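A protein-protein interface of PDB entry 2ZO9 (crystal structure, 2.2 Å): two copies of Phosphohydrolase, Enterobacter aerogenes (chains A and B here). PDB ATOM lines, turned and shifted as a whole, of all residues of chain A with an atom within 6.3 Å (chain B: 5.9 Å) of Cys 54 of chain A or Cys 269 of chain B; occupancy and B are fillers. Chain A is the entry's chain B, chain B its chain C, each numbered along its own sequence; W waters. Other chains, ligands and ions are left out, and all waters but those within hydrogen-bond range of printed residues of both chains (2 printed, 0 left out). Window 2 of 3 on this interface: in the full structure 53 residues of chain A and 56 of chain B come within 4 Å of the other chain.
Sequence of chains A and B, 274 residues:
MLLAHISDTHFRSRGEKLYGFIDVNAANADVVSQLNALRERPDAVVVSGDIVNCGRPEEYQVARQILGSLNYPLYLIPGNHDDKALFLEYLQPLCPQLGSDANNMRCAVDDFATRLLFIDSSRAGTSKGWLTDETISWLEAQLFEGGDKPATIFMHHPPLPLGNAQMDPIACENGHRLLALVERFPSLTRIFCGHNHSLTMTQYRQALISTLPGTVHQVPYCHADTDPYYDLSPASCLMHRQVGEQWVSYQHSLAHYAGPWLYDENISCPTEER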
ATOM      1  N   HIS A  10      24.139 -27.062 -25.311  1.00  0.00           N
ATOM      2  CA  HIS A  10      23.341 -26.967 -24.097  1.00  0.00           C
ATOM      3  C   HIS A  10      23.068 -28.273 -23.385  1.00  0.00           C
ATOM      4  O   HIS A  10      21.946 -28.477 -22.884  1.00  0.00           O
ATOM      5  CB  HIS A  10      22.007 -26.269 -24.375  1.00  0.00           C
ATOM      6  CG  HIS A  10      22.157 -24.797 -24.539  1.00  0.00           C
ATOM      7  ND1 HIS A  10      22.000 -23.915 -23.489  1.00  0.00           N
ATOM      8  CD2 HIS A  10      22.505 -24.050 -25.612  1.00  0.00           C
ATOM      9  CE1 HIS A  10      22.224 -22.688 -23.916  1.00  0.00           C
ATOM     10  NE2 HIS A  10      22.539 -22.745 -25.195  1.00  0.00           N
ATOM     11  N   PHE A  11      24.074 -29.148 -23.322  1.00  0.00           N
ATOM     12  CA  PHE A  11      23.927 -30.429 -22.624  1.00  0.00           C
ATOM     13  C   PHE A  11      23.319 -30.254 -21.217  1.00  0.00           C
ATOM     14  O   PHE A  11      23.609 -29.283 -20.526  1.00  0.00           O
ATOM     15  CB  PHE A  11      25.275 -31.156 -22.534  1.00  0.00           C
ATOM     16  CG  PHE A  11      25.743 -31.735 -23.846  1.00  0.00           C
ATOM     17  CD1 PHE A  11      26.758 -31.106 -24.586  1.00  0.00           C
ATOM     18  CD2 PHE A  11      25.176 -32.909 -24.357  1.00  0.00           C
ATOM     19  CE1 PHE A  11      27.194 -31.626 -25.787  1.00  0.00           C
ATOM     20  CE2 PHE A  11      25.614 -33.440 -25.554  1.00  0.00           C
ATOM     21  CZ  PHE A  11      26.642 -32.796 -26.277  1.00  0.00           C
ATOM     22  N   ARG A  12      22.475 -31.201 -20.817  1.00  0.00           N
ATOM     23  CA  ARG A  12      21.898 -31.263 -19.476  1.00  0.00           C
ATOM     24  C   ARG A  12      22.473 -32.492 -18.786  1.00  0.00           C
ATOM     25  O   ARG A  12      23.178 -33.278 -19.411  1.00  0.00           O
ATOM     26  CB  ARG A  12      20.358 -31.296 -19.544  1.00  0.00           C
ATOM     27  CG  ARG A  12      19.749 -29.966 -20.059  1.00  0.00           C
ATOM     28  CD  ARG A  12      19.391 -28.952 -18.954  1.00  0.00           C
ATOM     29  NE  ARG A  12      20.187 -29.238 -17.784  1.00  0.00           N
ATOM     30  CZ  ARG A  12      19.759 -29.640 -16.602  1.00  0.00           C
ATOM     31  NH1 ARG A  12      18.483 -29.730 -16.297  1.00  0.00           N
ATOM     32  NH2 ARG A  12      20.680 -29.904 -15.700  1.00  0.00           N
ATOM     33  N   TYR A  19      14.640 -27.549 -20.163  1.00  0.00           N
ATOM     34  CA  TYR A  19      13.283 -27.045 -19.812  1.00  0.00           C
ATOM     35  C   TYR A  19      12.295 -28.119 -19.425  1.00  0.00           C
ATOM     36  O   TYR A  19      11.076 -27.877 -19.362  1.00  0.00           O
ATOM     37  CB  TYR A  19      12.710 -26.119 -20.909  1.00  0.00           C
ATOM     38  CG  TYR A  19      13.758 -25.171 -21.478  1.00  0.00           C
ATOM     39  CD1 TYR A  19      13.786 -24.858 -22.833  1.00  0.00           C
ATOM     40  CD2 TYR A  19      14.745 -24.617 -20.656  1.00  0.00           C
ATOM     41  CE1 TYR A  19      14.764 -23.991 -23.359  1.00  0.00           C
ATOM     42  CE2 TYR A  19      15.708 -23.753 -21.156  1.00  0.00           C
ATOM     43  CZ  TYR A  19      15.714 -23.435 -22.502  1.00  0.00           C
ATOM     44  OH  TYR A  19      16.697 -22.576 -22.996  1.00  0.00           O
ATOM     45  N   VAL A  52      27.333 -26.710 -22.181  1.00  0.00           N
ATOM     46  CA  VAL A  52      26.351 -27.159 -21.197  1.00  0.00           C
ATOM     47  C   VAL A  52      25.360 -26.032 -20.900  1.00  0.00           C
ATOM     48  O   VAL A  52      25.618 -24.872 -21.228  1.00  0.00           O
ATOM     49  CB  VAL A  52      27.017 -27.653 -19.891  1.00  0.00           C
ATOM     50  CG1 VAL A  52      27.985 -28.808 -20.194  1.00  0.00           C
ATOM     51  CG2 VAL A  52      27.709 -26.511 -19.163  1.00  0.00           C
ATOM     52  N   ASN A  53      24.233 -26.374 -20.288  1.00  0.00           N
ATOM     53  CA  ASN A  53      23.207 -25.377 -20.022  1.00  0.00           C
ATOM     54  C   ASN A  53      23.359 -24.609 -18.687  1.00  0.00           C
ATOM     55  O   ASN A  53      23.062 -23.426 -18.607  1.00  0.00           O
ATOM     56  CB  ASN A  53      21.814 -25.993 -20.146  1.00  0.00           C
ATOM     57  CG  ASN A  53      20.727 -24.950 -20.191  1.00  0.00           C
ATOM     58  OD1 ASN A  53      20.666 -24.130 -21.123  1.00  0.00           O
ATOM     59  ND2 ASN A  53      19.868 -24.955 -19.185  1.00  0.00           N
ATOM     60  N   CYS A  54      23.859 -25.273 -17.657  1.00  0.00           N
ATOM     61  CA  CYS A  54      23.805 -24.719 -16.307  1.00  0.00           C
ATOM     62  C   CYS A  54      25.167 -24.578 -15.670  1.00  0.00           C
ATOM     63  O   CYS A  54      25.253 -24.155 -14.535  1.00  0.00           O
ATOM     64  CB  CYS A  54      22.935 -25.607 -15.412  1.00  0.00           C
ATOM     65  SG  CYS A  54      21.215 -25.677 -15.930  1.00  0.00           S
ATOM     66  N   GLY A  55      26.222 -24.954 -16.384  1.00  0.00           N
ATOM     67  CA  GLY A  55      27.583 -24.895 -15.854  1.00  0.00           C
ATOM     68  C   GLY A  55      27.779 -25.892 -14.733  1.00  0.00           C
ATOM     69  O   GLY A  55      28.549 -25.639 -13.833  1.00  0.00           O
ATOM     70  N   ARG A  56      27.068 -27.021 -14.774  1.00  0.00           N
ATOM     71  CA  ARG A  56      27.106 -28.044 -13.711  1.00  0.00           C
ATOM     72  C   ARG A  56      28.003 -29.221 -14.109  1.00  0.00           C
ATOM     73  O   ARG A  56      28.037 -29.581 -15.286  1.00  0.00           O
ATOM     74  CB  ARG A  56      25.684 -28.540 -13.408  1.00  0.00           C
ATOM     75  CG  ARG A  56      24.822 -27.501 -12.687  1.00  0.00           C
ATOM     76  CD  ARG A  56      23.366 -27.918 -12.648  1.00  0.00           C
ATOM     77  NE  ARG A  56      22.530 -26.855 -12.088  1.00  0.00           N
ATOM     78  CZ  ARG A  56      21.203 -26.921 -11.929  1.00  0.00           C
ATOM     79  NH1 ARG A  56      20.528 -27.999 -12.310  1.00  0.00           N
ATOM     80  NH2 ARG A  56      20.543 -25.887 -11.406  1.00  0.00           N
ATOM     81  N   GLU A  59      26.480 -32.092 -16.171  1.00  0.00           N
ATOM     82  CA  GLU A  59      26.295 -31.755 -17.588  1.00  0.00           C
ATOM     83  C   GLU A  59      27.598 -31.920 -18.357  1.00  0.00           C
ATOM     84  O   GLU A  59      27.598 -32.416 -19.488  1.00  0.00           O
ATOM     85  CB  GLU A  59      25.745 -30.347 -17.770  1.00  0.00           C
ATOM     86  CG  GLU A  59      24.542 -30.015 -16.916  1.00  0.00           C
ATOM     87  CD  GLU A  59      24.100 -28.555 -17.052  1.00  0.00           C
ATOM     88  OE1 GLU A  59      24.971 -27.678 -16.937  1.00  0.00           O
ATOM     89  OE2 GLU A  59      22.898 -28.275 -17.278  1.00  0.00           O
ATOM     90  N   HIS A  81      26.865 -19.869 -20.811  1.00  0.00           N
ATOM     91  CA  HIS A  81      26.248 -20.946 -20.021  1.00  0.00           C
ATOM     92  C   HIS A  81      27.256 -21.896 -19.391  1.00  0.00           C
ATOM     93  O   HIS A  81      26.902 -22.684 -18.514  1.00  0.00           O
ATOM     94  CB  HIS A  81      25.238 -21.714 -20.852  1.00  0.00           C
ATOM     95  CG  HIS A  81      23.936 -20.992 -21.029  1.00  0.00           C
ATOM     96  ND1 HIS A  81      22.788 -21.360 -20.360  1.00  0.00           N
ATOM     97  CD2 HIS A  81      23.605 -19.920 -21.786  1.00  0.00           C
ATOM     98  CE1 HIS A  81      21.803 -20.545 -20.701  1.00  0.00           C
ATOM     99  NE2 HIS A  81      22.277 -19.659 -21.557  1.00  0.00           N
ATOM    100  N   ASP A  82      28.504 -21.807 -19.843  1.00  0.00           N
ATOM    101  CA  ASP A  82      29.612 -22.616 -19.348  1.00  0.00           C
ATOM    102  C   ASP A  82      30.244 -22.053 -18.079  1.00  0.00           C
ATOM    103  O   ASP A  82      30.158 -20.847 -17.780  1.00  0.00           O
ATOM    104  CB  ASP A  82      30.697 -22.769 -20.432  1.00  0.00           C
ATOM    105  CG  ASP A  82      30.288 -23.743 -21.548  1.00  0.00           C
ATOM    106  OD1 ASP A  82      30.085 -24.949 -21.268  1.00  0.00           O
ATOM    107  OD2 ASP A  82      30.182 -23.312 -22.708  1.00  0.00           O
ATOM    108  N   ASP A  83      30.850 -22.959 -17.320  1.00  0.00           N
ATOM    109  CA  ASP A  83      31.709 -22.607 -16.213  1.00  0.00           C
ATOM    110  C   ASP A  83      33.146 -22.803 -16.661  1.00  0.00           C
ATOM    111  O   ASP A  83      33.502 -23.903 -17.071  1.00  0.00           O
ATOM    112  CB  ASP A  83      31.416 -23.512 -15.015  1.00  0.00           C
ATOM    113  CG  ASP A  83      32.155 -23.066 -13.767  1.00  0.00           C
ATOM    114  OD1 ASP A  83      31.728 -22.050 -13.171  1.00  0.00           O
ATOM    115  OD2 ASP A  83      33.170 -23.705 -13.391  1.00  0.00           O
ATOM    116  N   ASP B 264      12.793 -19.125 -19.254  1.00  0.00           N
ATOM    117  CA  ASP B 264      12.518 -18.862 -17.853  1.00  0.00           C
ATOM    118  C   ASP B 264      13.690 -19.500 -17.124  1.00  0.00           C
ATOM    119  O   ASP B 264      14.017 -20.662 -17.349  1.00  0.00           O
ATOM    120  CB  ASP B 264      11.160 -19.471 -17.441  1.00  0.00           C
ATOM    121  CG  ASP B 264      10.816 -19.256 -15.954  1.00  0.00           C
ATOM    122  OD1 ASP B 264      11.277 -20.042 -15.105  1.00  0.00           O
ATOM    123  OD2 ASP B 264      10.046 -18.331 -15.622  1.00  0.00           O
ATOM    124  N   GLU B 265      14.341 -18.716 -16.280  1.00  0.00           N
ATOM    125  CA  GLU B 265      15.589 -19.108 -15.620  1.00  0.00           C
ATOM    126  C   GLU B 265      15.410 -20.270 -14.648  1.00  0.00           C
ATOM    127  O   GLU B 265      16.323 -21.066 -14.467  1.00  0.00           O
ATOM    128  CB  GLU B 265      16.178 -17.908 -14.878  1.00  0.00           C
ATOM    129  CG  GLU B 265      17.616 -17.612 -15.234  1.00  0.00           C
ATOM    130  CD  GLU B 265      18.041 -16.190 -14.823  1.00  0.00           C
ATOM    131  OE1 GLU B 265      18.151 -15.917 -13.595  1.00  0.00           O
ATOM    132  OE2 GLU B 265      18.261 -15.345 -15.739  1.00  0.00           O
ATOM    133  N   ASN B 266      14.232 -20.358 -14.027  1.00  0.00           N
ATOM    134  CA  ASN B 266      13.918 -21.440 -13.087  1.00  0.00           C
ATOM    135  C   ASN B 266      13.698 -22.765 -13.809  1.00  0.00           C
ATOM    136  O   ASN B 266      14.075 -23.819 -13.310  1.00  0.00           O
ATOM    137  CB  ASN B 266      12.711 -21.076 -12.202  1.00  0.00           C
ATOM    138  CG  ASN B 266      12.209 -22.275 -11.335  1.00  0.00           C
ATOM    139  OD1 ASN B 266      12.853 -22.647 -10.324  1.00  0.00           O
ATOM    140  ND2 ASN B 266      11.044 -22.865 -11.718  1.00  0.00           N
ATOM    141  N   ILE B 267      13.077 -22.692 -14.979  1.00  0.00           N
ATOM    142  CA  ILE B 267      12.849 -23.843 -15.834  1.00  0.00           C
ATOM    143  C   ILE B 267      14.173 -24.261 -16.514  1.00  0.00           C
ATOM    144  O   ILE B 267      14.444 -25.450 -16.672  1.00  0.00           O
ATOM    145  CB  ILE B 267      11.713 -23.532 -16.867  1.00  0.00           C
ATOM    146  CG1 ILE B 267      10.352 -23.481 -16.141  1.00  0.00           C
ATOM    147  CG2 ILE B 267      11.723 -24.514 -18.036  1.00  0.00           C
ATOM    148  CD1 ILE B 267       9.203 -23.003 -16.985  1.00  0.00           C
ATOM    149  N   SER B 268      14.990 -23.289 -16.893  1.00  0.00           N
ATOM    150  CA  SER B 268      16.314 -23.562 -17.469  1.00  0.00           C
ATOM    151  C   SER B 268      17.231 -24.374 -16.547  1.00  0.00           C
ATOM    152  O   SER B 268      17.768 -25.399 -16.961  1.00  0.00           O
ATOM    153  CB  SER B 268      17.006 -22.258 -17.852  1.00  0.00           C
ATOM    154  OG  SER B 268      18.092 -22.509 -18.721  1.00  0.00           O
ATOM    155  N   CYS B 269      17.423 -23.894 -15.311  1.00  0.00           N
ATOM    156  CA  CYS B 269      18.272 -24.562 -14.323  1.00  0.00           C
ATOM    157  C   CYS B 269      17.531 -24.788 -12.998  1.00  0.00           C
ATOM    158  O   CYS B 269      17.662 -23.991 -12.072  1.00  0.00           O
ATOM    159  CB  CYS B 269      19.573 -23.787 -14.099  1.00  0.00           C
ATOM    160  SG  CYS B 269      20.599 -23.700 -15.613  1.00  0.00           S
ATOM    161  N   PRO B 270      16.760 -25.885 -12.909  1.00  0.00           N
ATOM    162  CA  PRO B 270      15.990 -26.215 -11.697  1.00  0.00           C
ATOM    163  C   PRO B 270      16.909 -26.580 -10.543  1.00  0.00           C
ATOM    164  O   PRO B 270      17.998 -27.080 -10.785  1.00  0.00           O
ATOM    165  CB  PRO B 270      15.160 -27.433 -12.120  1.00  0.00           C
ATOM    166  CG  PRO B 270      15.239 -27.477 -13.616  1.00  0.00           C
ATOM    167  CD  PRO B 270      16.568 -26.889 -13.973  1.00  0.00           C
ATOM    168  N   THR B 271      16.483 -26.327  -9.307  1.00  0.00           N
ATOM    169  CA  THR B 271      17.341 -26.559  -8.131  1.00  0.00           C
ATOM    170  C   THR B 271      16.865 -27.718  -7.245  1.00  0.00           C
ATOM    171  O   THR B 271      16.241 -28.674  -7.730  1.00  0.00           O
ATOM    172  CB  THR B 271      17.452 -25.290  -7.255  1.00  0.00           C
ATOM    173  OG1 THR B 271      16.141 -24.918  -6.815  1.00  0.00           O
ATOM    174  CG2 THR B 271      18.087 -24.117  -8.039  1.00  0.00           C
HETATM  175  O   HOH W   1      16.703 -27.490 -18.183  1.00  0.00           O
HETATM  176  O   HOH W   2      18.990 -22.240 -21.922  1.00  0.00           O
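No position is printed for both chains.
Among the printed residues, pairs that only touch across the chains: Tyr 19 of chain A with Ile 267 of chain B (3.4 Å), Tyr 19 of chain A with Ser 268 of chain B (3.6 Å), Asn 53 of chain A with Cys 269 of chain B (3.9 Å) and Arg 56 of chain A with Cys 269 of chain B (3.5 Å).
Printed residues of chain B that touch a printed residue of chain A: Ile 267, Ser 268, Cys 269 and Pro 270. Hydrophobic or aromatic side chains of chain B within 4 Å of the printed part of chain A: Ile 267. Hydrophobic or aromatic side chains of chain A that line the printed part of chain B: Tyr 19. Among the printed residues, 8 pairs touch across the chains. Among the printed residues, no Asp or Glu carboxylate lies within 4 Å of a Lys or Arg side-chain nitrogen of the other chain.
Cys 269 of chain B touches just these residues of chain A: Asn 53 (3.9 Å), Cys 54 (2.1 Å) and Arg 56 (3.5 Å). Printed residues of chain B within 4 Å of Tyr 19 of chain A: Ile 267 and Ser 268. Printed residues of chain B within 4 Å of Arg 56 of chain A: Cys 269 (3.5 Å) and Pro 270 (2.9 Å). The nearest residue of chain A that does not touch Cys 269 of chain B is Glu 59 of chain A (5.4 Å).
The side-chain amide nitrogen of Asn 53 of chain A is in hydrogen-bond range of the side-chain hydroxyl of Ser 268 of chain B (3.1 Å). The side-chain sulfur of Cys 54 of chain A is disulfide-bonded to the side-chain sulfur of Cys 269 of chain B (2.1 Å). The guanidinium group (NH2) of Arg 56 of chain A is in hydrogen-bond range of the backbone carbonyl oxygen (O) of Pro 270 of chain B, at 2.9 Å. O of Ser 268 of chain B sits close to SG of Cys 54 of chain A (3.6 Å).
Water W2 lies within hydrogen-bond range of the side-chain hydroxyl (OH) of Tyr 19 of chain A, the side-chain amide oxygen (OD1) of Asn 53 of chain A and the side-chain hydroxyl (OG) of Ser 268 of chain B. Water W1 lies within hydrogen-bond range of the backbone carbonyl oxygen of Ser 268 of chain B (2.6 Å), the backbone NH of Tyr 19 of chain A (2.9 Å), the backbone carbonyl oxygen of Ile 267 of chain B (3.4 Å) and the guanidinium group of Arg 12 of chain A (3.4 Å).
A ring nitrogen (ND1) of His 10 of chain A is in hydrogen-bond range of the side-chain amide oxygen (OD1) of Asn 53 of chain A. The backbone carbonyl oxygen (O) of Phe 11 of chain A lies within hydrogen-bond range of the backbone NH (N) of Asn 53 of chain A. SG of Cys 54 of chain A lies within hydrogen-bond range of ND2 of Asn 53 of chain A (3.6 Å). The backbone carbonyl oxygen (O) of Asn 53 of chain A sits at hydrogen-bond distance from a ring nitrogen (ND1) of His 81 of chain A (2.7 Å). The backbone NH (N) of Cys 54 of chain A is in hydrogen-bond range of the side-chain carboxylate (OE1) of Glu 59 of chain A (2.7 Å). N of Ile 267 of chain B is in hydrogen-bond range of OD1 of Asp 264 of chain B (3.2 Å).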
